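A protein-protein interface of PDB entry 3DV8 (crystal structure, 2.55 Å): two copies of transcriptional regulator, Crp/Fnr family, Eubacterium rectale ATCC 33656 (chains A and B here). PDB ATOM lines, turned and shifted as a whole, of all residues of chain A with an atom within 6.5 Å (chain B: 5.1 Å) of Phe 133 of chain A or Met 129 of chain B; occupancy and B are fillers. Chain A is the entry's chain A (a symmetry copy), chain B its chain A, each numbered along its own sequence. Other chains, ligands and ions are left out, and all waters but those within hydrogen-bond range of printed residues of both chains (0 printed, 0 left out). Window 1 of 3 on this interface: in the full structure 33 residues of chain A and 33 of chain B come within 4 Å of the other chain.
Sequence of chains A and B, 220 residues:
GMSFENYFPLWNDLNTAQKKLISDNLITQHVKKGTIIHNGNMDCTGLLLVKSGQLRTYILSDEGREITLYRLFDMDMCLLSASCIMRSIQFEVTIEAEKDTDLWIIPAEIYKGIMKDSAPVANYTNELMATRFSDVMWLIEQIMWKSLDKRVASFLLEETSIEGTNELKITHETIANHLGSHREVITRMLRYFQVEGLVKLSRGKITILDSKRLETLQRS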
ATOM      1  N   SER A  88     -26.514  19.457   2.847  1.00  0.00           N
ATOM      2  CA  SER A  88     -27.369  20.659   2.827  1.00  0.00           C
ATOM      3  C   SER A  88     -26.665  22.022   2.687  1.00  0.00           C
ATOM      4  O   SER A  88     -27.370  23.023   2.529  1.00  0.00           O
ATOM      5  CB  SER A  88     -28.310  20.674   4.032  1.00  0.00           C
ATOM      6  OG  SER A  88     -29.096  19.498   4.039  1.00  0.00           O
ATOM      7  N   ILE A  89     -25.324  22.080   2.775  1.00  0.00           N
ATOM      8  CA  ILE A  89     -24.577  23.336   2.512  1.00  0.00           C
ATOM      9  C   ILE A  89     -24.480  23.421   0.988  1.00  0.00           C
ATOM     10  O   ILE A  89     -23.640  22.768   0.390  1.00  0.00           O
ATOM     11  CB  ILE A  89     -23.138  23.385   3.140  1.00  0.00           C
ATOM     12  CG1 ILE A  89     -23.180  23.302   4.669  1.00  0.00           C
ATOM     13  CG2 ILE A  89     -22.400  24.669   2.710  1.00  0.00           C
ATOM     14  CD1 ILE A  89     -23.851  24.499   5.354  1.00  0.00           C
ATOM     15  N   THR A 125     -20.946  21.183  16.432  1.00  0.00           N
ATOM     16  CA  THR A 125     -20.919  21.644  15.042  1.00  0.00           C
ATOM     17  C   THR A 125     -22.119  22.562  14.730  1.00  0.00           C
ATOM     18  O   THR A 125     -21.965  23.505  13.942  1.00  0.00           O
ATOM     19  CB  THR A 125     -20.816  20.467  14.048  1.00  0.00           C
ATOM     20  OG1 THR A 125     -19.717  19.629  14.421  1.00  0.00           O
ATOM     21  CG2 THR A 125     -20.590  20.960  12.637  1.00  0.00           C
ATOM     22  N   ASN A 126     -23.285  22.292  15.344  1.00  0.00           N
ATOM     23  CA  ASN A 126     -24.483  23.170  15.250  1.00  0.00           C
ATOM     24  C   ASN A 126     -24.179  24.553  15.775  1.00  0.00           C
ATOM     25  O   ASN A 126     -24.473  25.548  15.113  1.00  0.00           O
ATOM     26  CB  ASN A 126     -25.686  22.635  16.059  1.00  0.00           C
ATOM     27  CG  ASN A 126     -26.437  21.547  15.344  1.00  0.00           C
ATOM     28  OD1 ASN A 126     -27.116  21.815  14.358  1.00  0.00           O
ATOM     29  ND2 ASN A 126     -26.367  20.319  15.854  1.00  0.00           N
ATOM     30  N   GLU A 127     -23.598  24.592  16.977  1.00  0.00           N
ATOM     31  CA  GLU A 127     -23.207  25.850  17.631  1.00  0.00           C
ATOM     32  C   GLU A 127     -22.163  26.619  16.809  1.00  0.00           C
ATOM     33  O   GLU A 127     -22.189  27.848  16.772  1.00  0.00           O
ATOM     34  CB  GLU A 127     -22.721  25.624  19.079  1.00  0.00           C
ATOM     35  CG  GLU A 127     -23.759  24.979  20.054  1.00  0.00           C
ATOM     36  CD  GLU A 127     -25.130  25.694  20.156  1.00  0.00           C
ATOM     37  OE1 GLU A 127     -25.205  26.924  19.932  1.00  0.00           O
ATOM     38  OE2 GLU A 127     -26.138  25.010  20.493  1.00  0.00           O
ATOM     39  N   LEU A 128     -21.288  25.886  16.122  1.00  0.00           N
ATOM     40  CA  LEU A 128     -20.277  26.472  15.247  1.00  0.00           C
ATOM     41  C   LEU A 128     -20.979  27.072  14.012  1.00  0.00           C
ATOM     42  O   LEU A 128     -20.694  28.215  13.650  1.00  0.00           O
ATOM     43  CB  LEU A 128     -19.225  25.421  14.872  1.00  0.00           C
ATOM     44  CG  LEU A 128     -17.885  25.892  14.328  1.00  0.00           C
ATOM     45  CD1 LEU A 128     -17.170  26.818  15.324  1.00  0.00           C
ATOM     46  CD2 LEU A 128     -17.035  24.665  14.010  1.00  0.00           C
ATOM     47  N   MET A 129     -21.895  26.311  13.395  1.00  0.00           N
ATOM     48  CA  MET A 129     -22.730  26.823  12.273  1.00  0.00           C
ATOM     49  C   MET A 129     -23.585  28.029  12.650  1.00  0.00           C
ATOM     50  O   MET A 129     -23.647  28.981  11.885  1.00  0.00           O
ATOM     51  CB  MET A 129     -23.689  25.770  11.677  1.00  0.00           C
ATOM     52  CG  MET A 129     -23.350  25.291  10.282  1.00  0.00           C
ATOM     53  SD  MET A 129     -24.940  24.562   9.449  1.00  0.00           S
ATOM     54  CE  MET A 129     -25.341  23.266  10.706  1.00  0.00           C
ATOM     55  N   ALA A 130     -24.275  27.943  13.791  1.00  0.00           N
ATOM     56  CA  ALA A 130     -25.116  29.026  14.309  1.00  0.00           C
ATOM     57  C   ALA A 130     -24.335  30.338  14.472  1.00  0.00           C
ATOM     58  O   ALA A 130     -24.846  31.395  14.118  1.00  0.00           O
ATOM     59  CB  ALA A 130     -25.773  28.613  15.632  1.00  0.00           C
ATOM     60  N   THR A 131     -23.098  30.251  14.976  1.00  0.00           N
ATOM     61  CA  THR A 131     -22.192  31.410  15.114  1.00  0.00           C
ATOM     62  C   THR A 131     -21.916  32.073  13.758  1.00  0.00           C
ATOM     63  O   THR A 131     -22.036  33.292  13.626  1.00  0.00           O
ATOM     64  CB  THR A 131     -20.821  31.003  15.727  1.00  0.00           C
ATOM     65  OG1 THR A 131     -21.039  30.324  16.965  1.00  0.00           O
ATOM     66  CG2 THR A 131     -19.929  32.214  15.972  1.00  0.00           C
ATOM     67  N   ARG A 132     -21.579  31.252  12.762  1.00  0.00           N
ATOM     68  CA  ARG A 132     -21.273  31.722  11.398  1.00  0.00           C
ATOM     69  C   ARG A 132     -22.564  32.217  10.705  1.00  0.00           C
ATOM     70  O   ARG A 132     -22.525  33.214   9.980  1.00  0.00           O
ATOM     71  CB  ARG A 132     -20.552  30.634  10.581  1.00  0.00           C
ATOM     72  CG  ARG A 132     -19.267  30.047  11.251  1.00  0.00           C
ATOM     73  CD  ARG A 132     -18.054  30.963  11.296  1.00  0.00           C
ATOM     74  NE  ARG A 132     -17.052  30.499  12.284  1.00  0.00           N
ATOM     75  CZ  ARG A 132     -16.832  31.021  13.500  1.00  0.00           C
ATOM     76  NH1 ARG A 132     -17.495  32.089  13.954  1.00  0.00           N
ATOM     77  NH2 ARG A 132     -15.904  30.492  14.296  1.00  0.00           N
ATOM     78  N   PHE A 133     -23.691  31.529  10.953  1.00  0.00           N
ATOM     79  CA  PHE A 133     -25.026  31.941  10.463  1.00  0.00           C
ATOM     80  C   PHE A 133     -25.307  33.329  11.055  1.00  0.00           C
ATOM     81  O   PHE A 133     -25.680  34.241  10.319  1.00  0.00           O
ATOM     82  CB  PHE A 133     -26.126  30.964  10.929  1.00  0.00           C
ATOM     83  CG  PHE A 133     -27.409  30.962  10.094  1.00  0.00           C
ATOM     84  CD1 PHE A 133     -27.870  32.073   9.369  1.00  0.00           C
ATOM     85  CD2 PHE A 133     -28.222  29.821  10.134  1.00  0.00           C
ATOM     86  CE1 PHE A 133     -29.060  32.013   8.649  1.00  0.00           C
ATOM     87  CE2 PHE A 133     -29.418  29.757   9.432  1.00  0.00           C
ATOM     88  CZ  PHE A 133     -29.845  30.853   8.689  1.00  0.00           C
ATOM     89  N   SER A 134     -25.098  33.479  12.371  1.00  0.00           N
ATOM     90  CA  SER A 134     -25.279  34.769  13.053  1.00  0.00           C
ATOM     91  C   SER A 134     -24.355  35.861  12.474  1.00  0.00           C
ATOM     92  O   SER A 134     -24.824  36.982  12.274  1.00  0.00           O
ATOM     93  CB  SER A 134     -25.084  34.653  14.572  1.00  0.00           C
ATOM     94  OG  SER A 134     -25.958  33.698  15.146  1.00  0.00           O
ATOM     95  N   ASP A 135     -23.083  35.529  12.182  1.00  0.00           N
ATOM     96  CA  ASP A 135     -22.123  36.477  11.549  1.00  0.00           C
ATOM     97  C   ASP A 135     -22.676  36.996  10.214  1.00  0.00           C
ATOM     98  O   ASP A 135     -22.707  38.206   9.962  1.00  0.00           O
ATOM     99  CB  ASP A 135     -20.746  35.829  11.260  1.00  0.00           C
ATOM    100  CG  ASP A 135     -19.966  35.448  12.517  1.00  0.00           C
ATOM    101  OD1 ASP A 135     -20.214  36.022  13.593  1.00  0.00           O
ATOM    102  OD2 ASP A 135     -19.068  34.580  12.418  1.00  0.00           O
ATOM    103  N   VAL A 136     -23.111  36.061   9.372  1.00  0.00           N
ATOM    104  CA  VAL A 136     -23.723  36.379   8.081  1.00  0.00           C
ATOM    105  C   VAL A 136     -25.046  37.168   8.226  1.00  0.00           C
ATOM    106  O   VAL A 136     -25.363  37.993   7.371  1.00  0.00           O
ATOM    107  CB  VAL A 136     -23.897  35.095   7.227  1.00  0.00           C
ATOM    108  CG1 VAL A 136     -24.731  35.358   6.015  1.00  0.00           C
ATOM    109  CG2 VAL A 136     -22.518  34.537   6.826  1.00  0.00           C
ATOM    110  N   MET A 137     -25.805  36.928   9.294  1.00  0.00           N
ATOM    111  CA  MET A 137     -27.041  37.711   9.553  1.00  0.00           C
ATOM    112  C   MET A 137     -26.765  39.151   9.983  1.00  0.00           C
ATOM    113  O   MET A 137     -27.568  40.035   9.665  1.00  0.00           O
ATOM    114  CB  MET A 137     -27.961  36.998  10.537  1.00  0.00           C
ATOM    115  CG  MET A 137     -28.595  35.737   9.972  1.00  0.00           C
ATOM    116  SD  MET A 137     -30.036  36.098   8.740  1.00  0.00           S
ATOM    117  CE  MET A 137     -29.064  36.519   7.302  1.00  0.00           C
ATOM    118  N   TRP A 138     -25.663  39.376  10.714  1.00  0.00           N
ATOM    119  CA  TRP A 138     -25.216  40.733  11.044  1.00  0.00           C
ATOM    120  C   TRP A 138     -24.826  41.456   9.743  1.00  0.00           C
ATOM    121  O   TRP A 138     -25.101  42.657   9.603  1.00  0.00           O
ATOM    122  CB  TRP A 138     -24.061  40.749  12.059  1.00  0.00           C
ATOM    123  CG  TRP A 138     -23.386  42.099  12.165  1.00  0.00           C
ATOM    124  CD1 TRP A 138     -23.832  43.199  12.852  1.00  0.00           C
ATOM    125  CD2 TRP A 138     -22.152  42.492  11.532  1.00  0.00           C
ATOM    126  NE1 TRP A 138     -22.950  44.251  12.689  1.00  0.00           N
ATOM    127  CE2 TRP A 138     -21.913  43.847  11.886  1.00  0.00           C
ATOM    128  CE3 TRP A 138     -21.222  41.828  10.700  1.00  0.00           C
ATOM    129  CZ2 TRP A 138     -20.772  44.552  11.441  1.00  0.00           C
ATOM    130  CZ3 TRP A 138     -20.087  42.531  10.247  1.00  0.00           C
ATOM    131  CH2 TRP A 138     -19.875  43.881  10.624  1.00  0.00           C
ATOM    132  N   LEU B  79     -37.054  25.659  12.032  1.00  0.00           N
ATOM    133  CA  LEU B  79     -36.106  25.493  13.139  1.00  0.00           C
ATOM    134  C   LEU B  79     -36.009  26.753  13.994  1.00  0.00           C
ATOM    135  O   LEU B  79     -35.987  26.653  15.227  1.00  0.00           O
ATOM    136  CB  LEU B  79     -34.706  25.133  12.616  1.00  0.00           C
ATOM    137  CG  LEU B  79     -33.557  24.930  13.623  1.00  0.00           C
ATOM    138  CD1 LEU B  79     -33.939  23.990  14.763  1.00  0.00           C
ATOM    139  CD2 LEU B  79     -32.320  24.402  12.918  1.00  0.00           C
ATOM    140  N   LEU B  80     -35.974  27.925  13.337  1.00  0.00           N
ATOM    141  CA  LEU B  80     -35.757  29.234  14.005  1.00  0.00           C
ATOM    142  C   LEU B  80     -36.880  29.730  14.926  1.00  0.00           C
ATOM    143  O   LEU B  80     -36.687  30.702  15.668  1.00  0.00           O
ATOM    144  CB  LEU B  80     -35.339  30.312  12.989  1.00  0.00           C
ATOM    145  CG  LEU B  80     -34.111  29.981  12.119  1.00  0.00           C
ATOM    146  CD1 LEU B  80     -33.825  31.129  11.153  1.00  0.00           C
ATOM    147  CD2 LEU B  80     -32.866  29.647  12.948  1.00  0.00           C
ATOM    148  N   MET B  86     -30.589  26.957  20.976  1.00  0.00           N
ATOM    149  CA  MET B  86     -29.187  27.084  20.547  1.00  0.00           C
ATOM    150  C   MET B  86     -28.650  28.453  20.943  1.00  0.00           C
ATOM    151  O   MET B  86     -29.026  29.460  20.344  1.00  0.00           O
ATOM    152  CB  MET B  86     -29.091  26.903  19.040  1.00  0.00           C
ATOM    153  CG  MET B  86     -29.351  25.475  18.605  1.00  0.00           C
ATOM    154  SD  MET B  86     -30.246  25.391  16.886  1.00  0.00           S
ATOM    155  CE  MET B  86     -32.004  26.324  17.232  1.00  0.00           C
ATOM    156  N   ILE B  89     -27.248  31.054  18.222  1.00  0.00           N
ATOM    157  CA  ILE B  89     -28.128  31.812  17.298  1.00  0.00           C
ATOM    158  C   ILE B  89     -28.321  33.172  17.971  1.00  0.00           C
ATOM    159  O   ILE B  89     -29.126  33.298  18.880  1.00  0.00           O
ATOM    160  CB  ILE B  89     -29.526  31.146  17.033  1.00  0.00           C
ATOM    161  CG1 ILE B  89     -29.389  29.778  16.360  1.00  0.00           C
ATOM    162  CG2 ILE B  89     -30.411  32.065  16.165  1.00  0.00           C
ATOM    163  CD1 ILE B  89     -28.799  29.821  14.944  1.00  0.00           C
ATOM    164  N   PHE B  91     -29.228  36.156  16.485  1.00  0.00           N
ATOM    165  CA  PHE B  91     -30.033  37.032  15.621  1.00  0.00           C
ATOM    166  C   PHE B  91     -31.495  36.647  15.800  1.00  0.00           C
ATOM    167  O   PHE B  91     -31.815  35.477  16.073  1.00  0.00           O
ATOM    168  CB  PHE B  91     -29.633  36.932  14.141  1.00  0.00           C
ATOM    169  CG  PHE B  91     -29.829  35.564  13.528  1.00  0.00           C
ATOM    170  CD1 PHE B  91     -28.889  34.550  13.738  1.00  0.00           C
ATOM    171  CD2 PHE B  91     -30.932  35.294  12.715  1.00  0.00           C
ATOM    172  CE1 PHE B  91     -29.046  33.267  13.157  1.00  0.00           C
ATOM    173  CE2 PHE B  91     -31.111  34.016  12.120  1.00  0.00           C
ATOM    174  CZ  PHE B  91     -30.168  33.001  12.343  1.00  0.00           C
ATOM    175  N   THR B 125     -30.719  18.286  12.615  1.00  0.00           N
ATOM    176  CA  THR B 125     -30.872  19.716  12.891  1.00  0.00           C
ATOM    177  C   THR B 125     -29.787  20.547  12.173  1.00  0.00           C
ATOM    178  O   THR B 125     -30.078  21.671  11.744  1.00  0.00           O
ATOM    179  CB  THR B 125     -30.916  20.008  14.407  1.00  0.00           C
ATOM    180  OG1 THR B 125     -31.904  19.173  15.020  1.00  0.00           O
ATOM    181  CG2 THR B 125     -31.270  21.453  14.677  1.00  0.00           C
ATOM    182  N   ASN B 126     -28.567  19.997  12.042  1.00  0.00           N
ATOM    183  CA  ASN B 126     -27.469  20.618  11.254  1.00  0.00           C
ATOM    184  C   ASN B 126     -27.876  20.793   9.810  1.00  0.00           C
ATOM    185  O   ASN B 126     -27.720  21.877   9.248  1.00  0.00           O
ATOM    186  CB  ASN B 126     -26.175  19.774  11.257  1.00  0.00           C
ATOM    187  CG  ASN B 126     -25.362  19.948  12.510  1.00  0.00           C
ATOM    188  OD1 ASN B 126     -24.772  21.003  12.716  1.00  0.00           O
ATOM    189  ND2 ASN B 126     -25.282  18.907  13.336  1.00  0.00           N
ATOM    190  N   GLU B 127     -28.387  19.707   9.225  1.00  0.00           N
ATOM    191  CA  GLU B 127     -28.862  19.702   7.832  1.00  0.00           C
ATOM    192  C   GLU B 127     -30.022  20.685   7.622  1.00  0.00           C
ATOM    193  O   GLU B 127     -30.119  21.310   6.567  1.00  0.00           O
ATOM    194  CB  GLU B 127     -29.239  18.283   7.353  1.00  0.00           C
ATOM    195  CG  GLU B 127     -28.088  17.225   7.382  1.00  0.00           C
ATOM    196  CD  GLU B 127     -26.790  17.615   6.630  1.00  0.00           C
ATOM    197  OE1 GLU B 127     -26.850  18.408   5.662  1.00  0.00           O
ATOM    198  OE2 GLU B 127     -25.701  17.092   7.004  1.00  0.00           O
ATOM    199  N   LEU B 128     -30.859  20.847   8.647  1.00  0.00           N
ATOM    200  CA  LEU B 128     -31.972  21.791   8.619  1.00  0.00           C
ATOM    201  C   LEU B 128     -31.405  23.225   8.656  1.00  0.00           C
ATOM    202  O   LEU B 128     -31.820  24.061   7.852  1.00  0.00           O
ATOM    203  CB  LEU B 128     -32.936  21.511   9.779  1.00  0.00           C
ATOM    204  CG  LEU B 128     -34.344  22.080   9.711  1.00  0.00           C
ATOM    205  CD1 LEU B 128     -35.088  21.585   8.461  1.00  0.00           C
ATOM    206  CD2 LEU B 128     -35.087  21.684  10.984  1.00  0.00           C
ATOM    207  N   MET B 129     -30.455  23.488   9.567  1.00  0.00           N
ATOM    208  CA  MET B 129     -29.741  24.793   9.618  1.00  0.00           C
ATOM    209  C   MET B 129     -28.989  25.127   8.334  1.00  0.00           C
ATOM    210  O   MET B 129     -29.064  26.257   7.872  1.00  0.00           O
ATOM    211  CB  MET B 129     -28.720  24.902  10.771  1.00  0.00           C
ATOM    212  CG  MET B 129     -29.090  25.856  11.886  1.00  0.00           C
ATOM    213  SD  MET B 129     -27.487  26.387  12.835  1.00  0.00           S
ATOM    214  CE  MET B 129     -26.888  24.709  13.330  1.00  0.00           C
ATOM    215  N   ALA B 130     -28.229  24.159   7.814  1.00  0.00           N
ATOM    216  CA  ALA B 130     -27.469  24.309   6.569  1.00  0.00           C
ATOM    217  C   ALA B 130     -28.364  24.721   5.391  1.00  0.00           C
ATOM    218  O   ALA B 130     -27.981  25.586   4.613  1.00  0.00           O
ATOM    219  CB  ALA B 130     -26.699  23.023   6.248  1.00  0.00           C
ATOM    220  N   THR B 131     -29.555  24.118   5.293  1.00  0.00           N
ATOM    221  CA  THR B 131     -30.562  24.465   4.268  1.00  0.00           C
ATOM    222  C   THR B 131     -30.980  25.938   4.365  1.00  0.00           C
ATOM    223  O   THR B 131     -30.987  26.650   3.360  1.00  0.00           O
ATOM    224  CB  THR B 131     -31.848  23.600   4.404  1.00  0.00           C
ATOM    225  OG1 THR B 131     -31.494  22.217   4.382  1.00  0.00           O
ATOM    226  CG2 THR B 131     -32.839  23.880   3.281  1.00  0.00           C
ATOM    227  N   ARG B 132     -31.291  26.379   5.586  1.00  0.00           N
ATOM    228  CA  ARG B 132     -31.720  27.764   5.856  1.00  0.00           C
ATOM    229  C   ARG B 132     -30.526  28.733   5.687  1.00  0.00           C
ATOM    230  O   ARG B 132     -30.705  29.839   5.173  1.00  0.00           O
ATOM    231  CB  ARG B 132     -32.377  27.883   7.245  1.00  0.00           C
ATOM    232  CG  ARG B 132     -33.557  26.891   7.504  1.00  0.00           C
ATOM    233  CD  ARG B 132     -34.850  27.172   6.755  1.00  0.00           C
ATOM    234  NE  ARG B 132     -35.743  25.990   6.737  1.00  0.00           N
ATOM    235  CZ  ARG B 132     -35.942  25.158   5.703  1.00  0.00           C
ATOM    236  NH1 ARG B 132     -35.362  25.340   4.512  1.00  0.00           N
ATOM    237  NH2 ARG B 132     -36.766  24.119   5.830  1.00  0.00           N
ATOM    238  N   PHE B 133     -29.324  28.297   6.101  1.00  0.00           N
ATOM    239  CA  PHE B 133     -28.067  29.053   5.903  1.00  0.00           C
ATOM    240  C   PHE B 133     -27.890  29.230   4.389  1.00  0.00           C
ATOM    241  O   PHE B 133     -27.651  30.345   3.930  1.00  0.00           O
ATOM    242  CB  PHE B 133     -26.851  28.285   6.464  1.00  0.00           C
ATOM    243  CG  PHE B 133     -25.625  29.138   6.799  1.00  0.00           C
ATOM    244  CD1 PHE B 133     -25.318  30.349   6.156  1.00  0.00           C
ATOM    245  CD2 PHE B 133     -24.703  28.636   7.726  1.00  0.00           C
ATOM    246  CE1 PHE B 133     -24.172  31.065   6.489  1.00  0.00           C
ATOM    247  CE2 PHE B 133     -23.549  29.335   8.055  1.00  0.00           C
ATOM    248  CZ  PHE B 133     -23.275  30.551   7.436  1.00  0.00           C
ATOM    249  N   SER B 134     -28.036  28.134   3.630  1.00  0.00           N
ATOM    250  CA  SER B 134     -27.944  28.176   2.163  1.00  0.00           C
ATOM    251  C   SER B 134     -29.003  29.114   1.546  1.00  0.00           C
ATOM    252  O   SER B 134     -28.658  29.872   0.639  1.00  0.00           O
ATOM    253  CB  SER B 134     -28.038  26.777   1.537  1.00  0.00           C
ATOM    254  OG  SER B 134     -27.043  25.904   2.040  1.00  0.00           O
ATOM    255  N   VAL B 136     -30.437  31.792   2.953  1.00  0.00           N
ATOM    256  CA  VAL B 136     -29.935  33.131   3.268  1.00  0.00           C
ATOM    257  C   VAL B 136     -28.691  33.513   2.433  1.00  0.00           C
ATOM    258  O   VAL B 136     -28.505  34.685   2.110  1.00  0.00           O
ATOM    259  CB  VAL B 136     -29.686  33.276   4.793  1.00  0.00           C
ATOM    260  CG1 VAL B 136     -28.953  34.541   5.104  1.00  0.00           C
ATOM    261  CG2 VAL B 136     -31.024  33.223   5.554  1.00  0.00           C
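Of the 16 printed residues of chain A, 12 touch a printed residue of chain B. Printed residues of chain A that touch a printed residue of chain B: Ser 88, Ile 89, Thr 125, Asn 126, Glu 127, Met 129, Ala 130, Arg 132, Phe 133, Ser 134, Val 136 and Met 137. Hydrophobic or aromatic side chains of chain A that line the printed part of chain B: Ile 89, Met 129, Ala 130, Phe 133, Val 136 and Met 137. Of the 16 printed residues of chain B, 13 touch a printed residue of chain A. Hydrophobic or aromatic side chains of chain B that line the printed part of chain A: Met 86, Ile 89, Phe 91, Met 129, Ala 130, Phe 133 and Val 136.
OG1 of Thr 131 of chain B touches CB of Ser 88 of chain A (3.6 Å). Ser 134 of chain B touches Ile 89 of chain A (OG to CA, 3.6 Å). Thr 125 of chain A touches Asn 126 of chain B. Glu 127 of chain A touches Met 86 of chain B. Phe 133 of chain B touches Met 129 of chain A. Ala 130 of chain A touches Ile 89 of chain B (CB to CD1, 3.3 Å). Phe 91 of chain B touches Phe 133 of chain A. CZ of Phe 133 of chain A touches C of Arg 132 of chain B, at 3.7 Å. Ile 89 of chain B touches Ser 134 of chain A. Val 136 of chain A touches Phe 133 of chain B.
Thr 125 of chain A touches Asn 126 of chain B, and with the chains exchanged Asn 126 of chain A touches Thr 125 of chain B. Asn 126 of chain B touches its own counterpart, Asn 126 of chain A. Arg 132 of chain A touches Phe 133 of chain B, and with the chains exchanged Phe 133 of chain A touches Arg 132 of chain B. Phe 133 of chain A touches its own counterpart, Phe 133 of chain B. 12 positions are printed for both chains. Of the 28 pairs that touch across the chains among the printed residues, 19 have their exchanged pair printed and touching as well.
Of the printed residues of chain B, Glu 127 of chain A touches Met 86. Leu 128 of chain A touches none of the printed residues of chain B. Of the printed residues of chain A, Met 86 of chain B touches Glu 127. Met 129 of chain B touches four residues of chain A. Of the printed residues of chain A, Arg 132 of chain B touches Phe 133. Of the printed residues of chain A, Val 136 of chain B touches Phe 133 and Met 137.
The side-chain amide oxygen of Asn 126 of chain B lies close to the side-chain amide oxygen of Asn 126 of chain A (3.0 Å). OG of Ser 88 of chain A lies within hydrogen-bond range of OE1 of Glu 127 of chain B, 3.0 Å away. SD of Met 129 of chain B is in hydrogen-bond range of N of Ala 130 of chain A (3.7 Å). The backbone NH (N) of Ala 130 of chain B is in hydrogen-bond range of the side-chain sulfur (SD) of Met 129 of chain A, 3.7 Å away. The side-chain hydroxyl of Ser 134 of chain B lies within hydrogen-bond range of the backbone carbonyl oxygen of Ser 88 of chain A (2.9 Å). The backbone carbonyl oxygen of Ala 130 of chain B lies close to the backbone carbonyl oxygen of Ser 88 of chain A.
The backbone carbonyl oxygen (O) of Glu 127 of chain B lies within hydrogen-bond range of the side-chain hydroxyl (OG1) of Thr 131 of chain B (2.7 Å). The backbone carbonyl oxygen (O) of Ala 130 of chain B is in hydrogen-bond range of the side-chain hydroxyl (OG) of Ser 134 of chain B, at 2.8 Å. O of Glu 127 of chain A lies within hydrogen-bond range of OG1 of Thr 131 of chain A, at 2.7 Å. OG of Ser 134 of chain A lies within hydrogen-bond range of O of Ala 130 of chain A, at 2.8 Å. NH1 of Arg 132 of chain A lies within salt-bridge range of OD2 of Asp 135 of chain A, at 3.3 Å.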
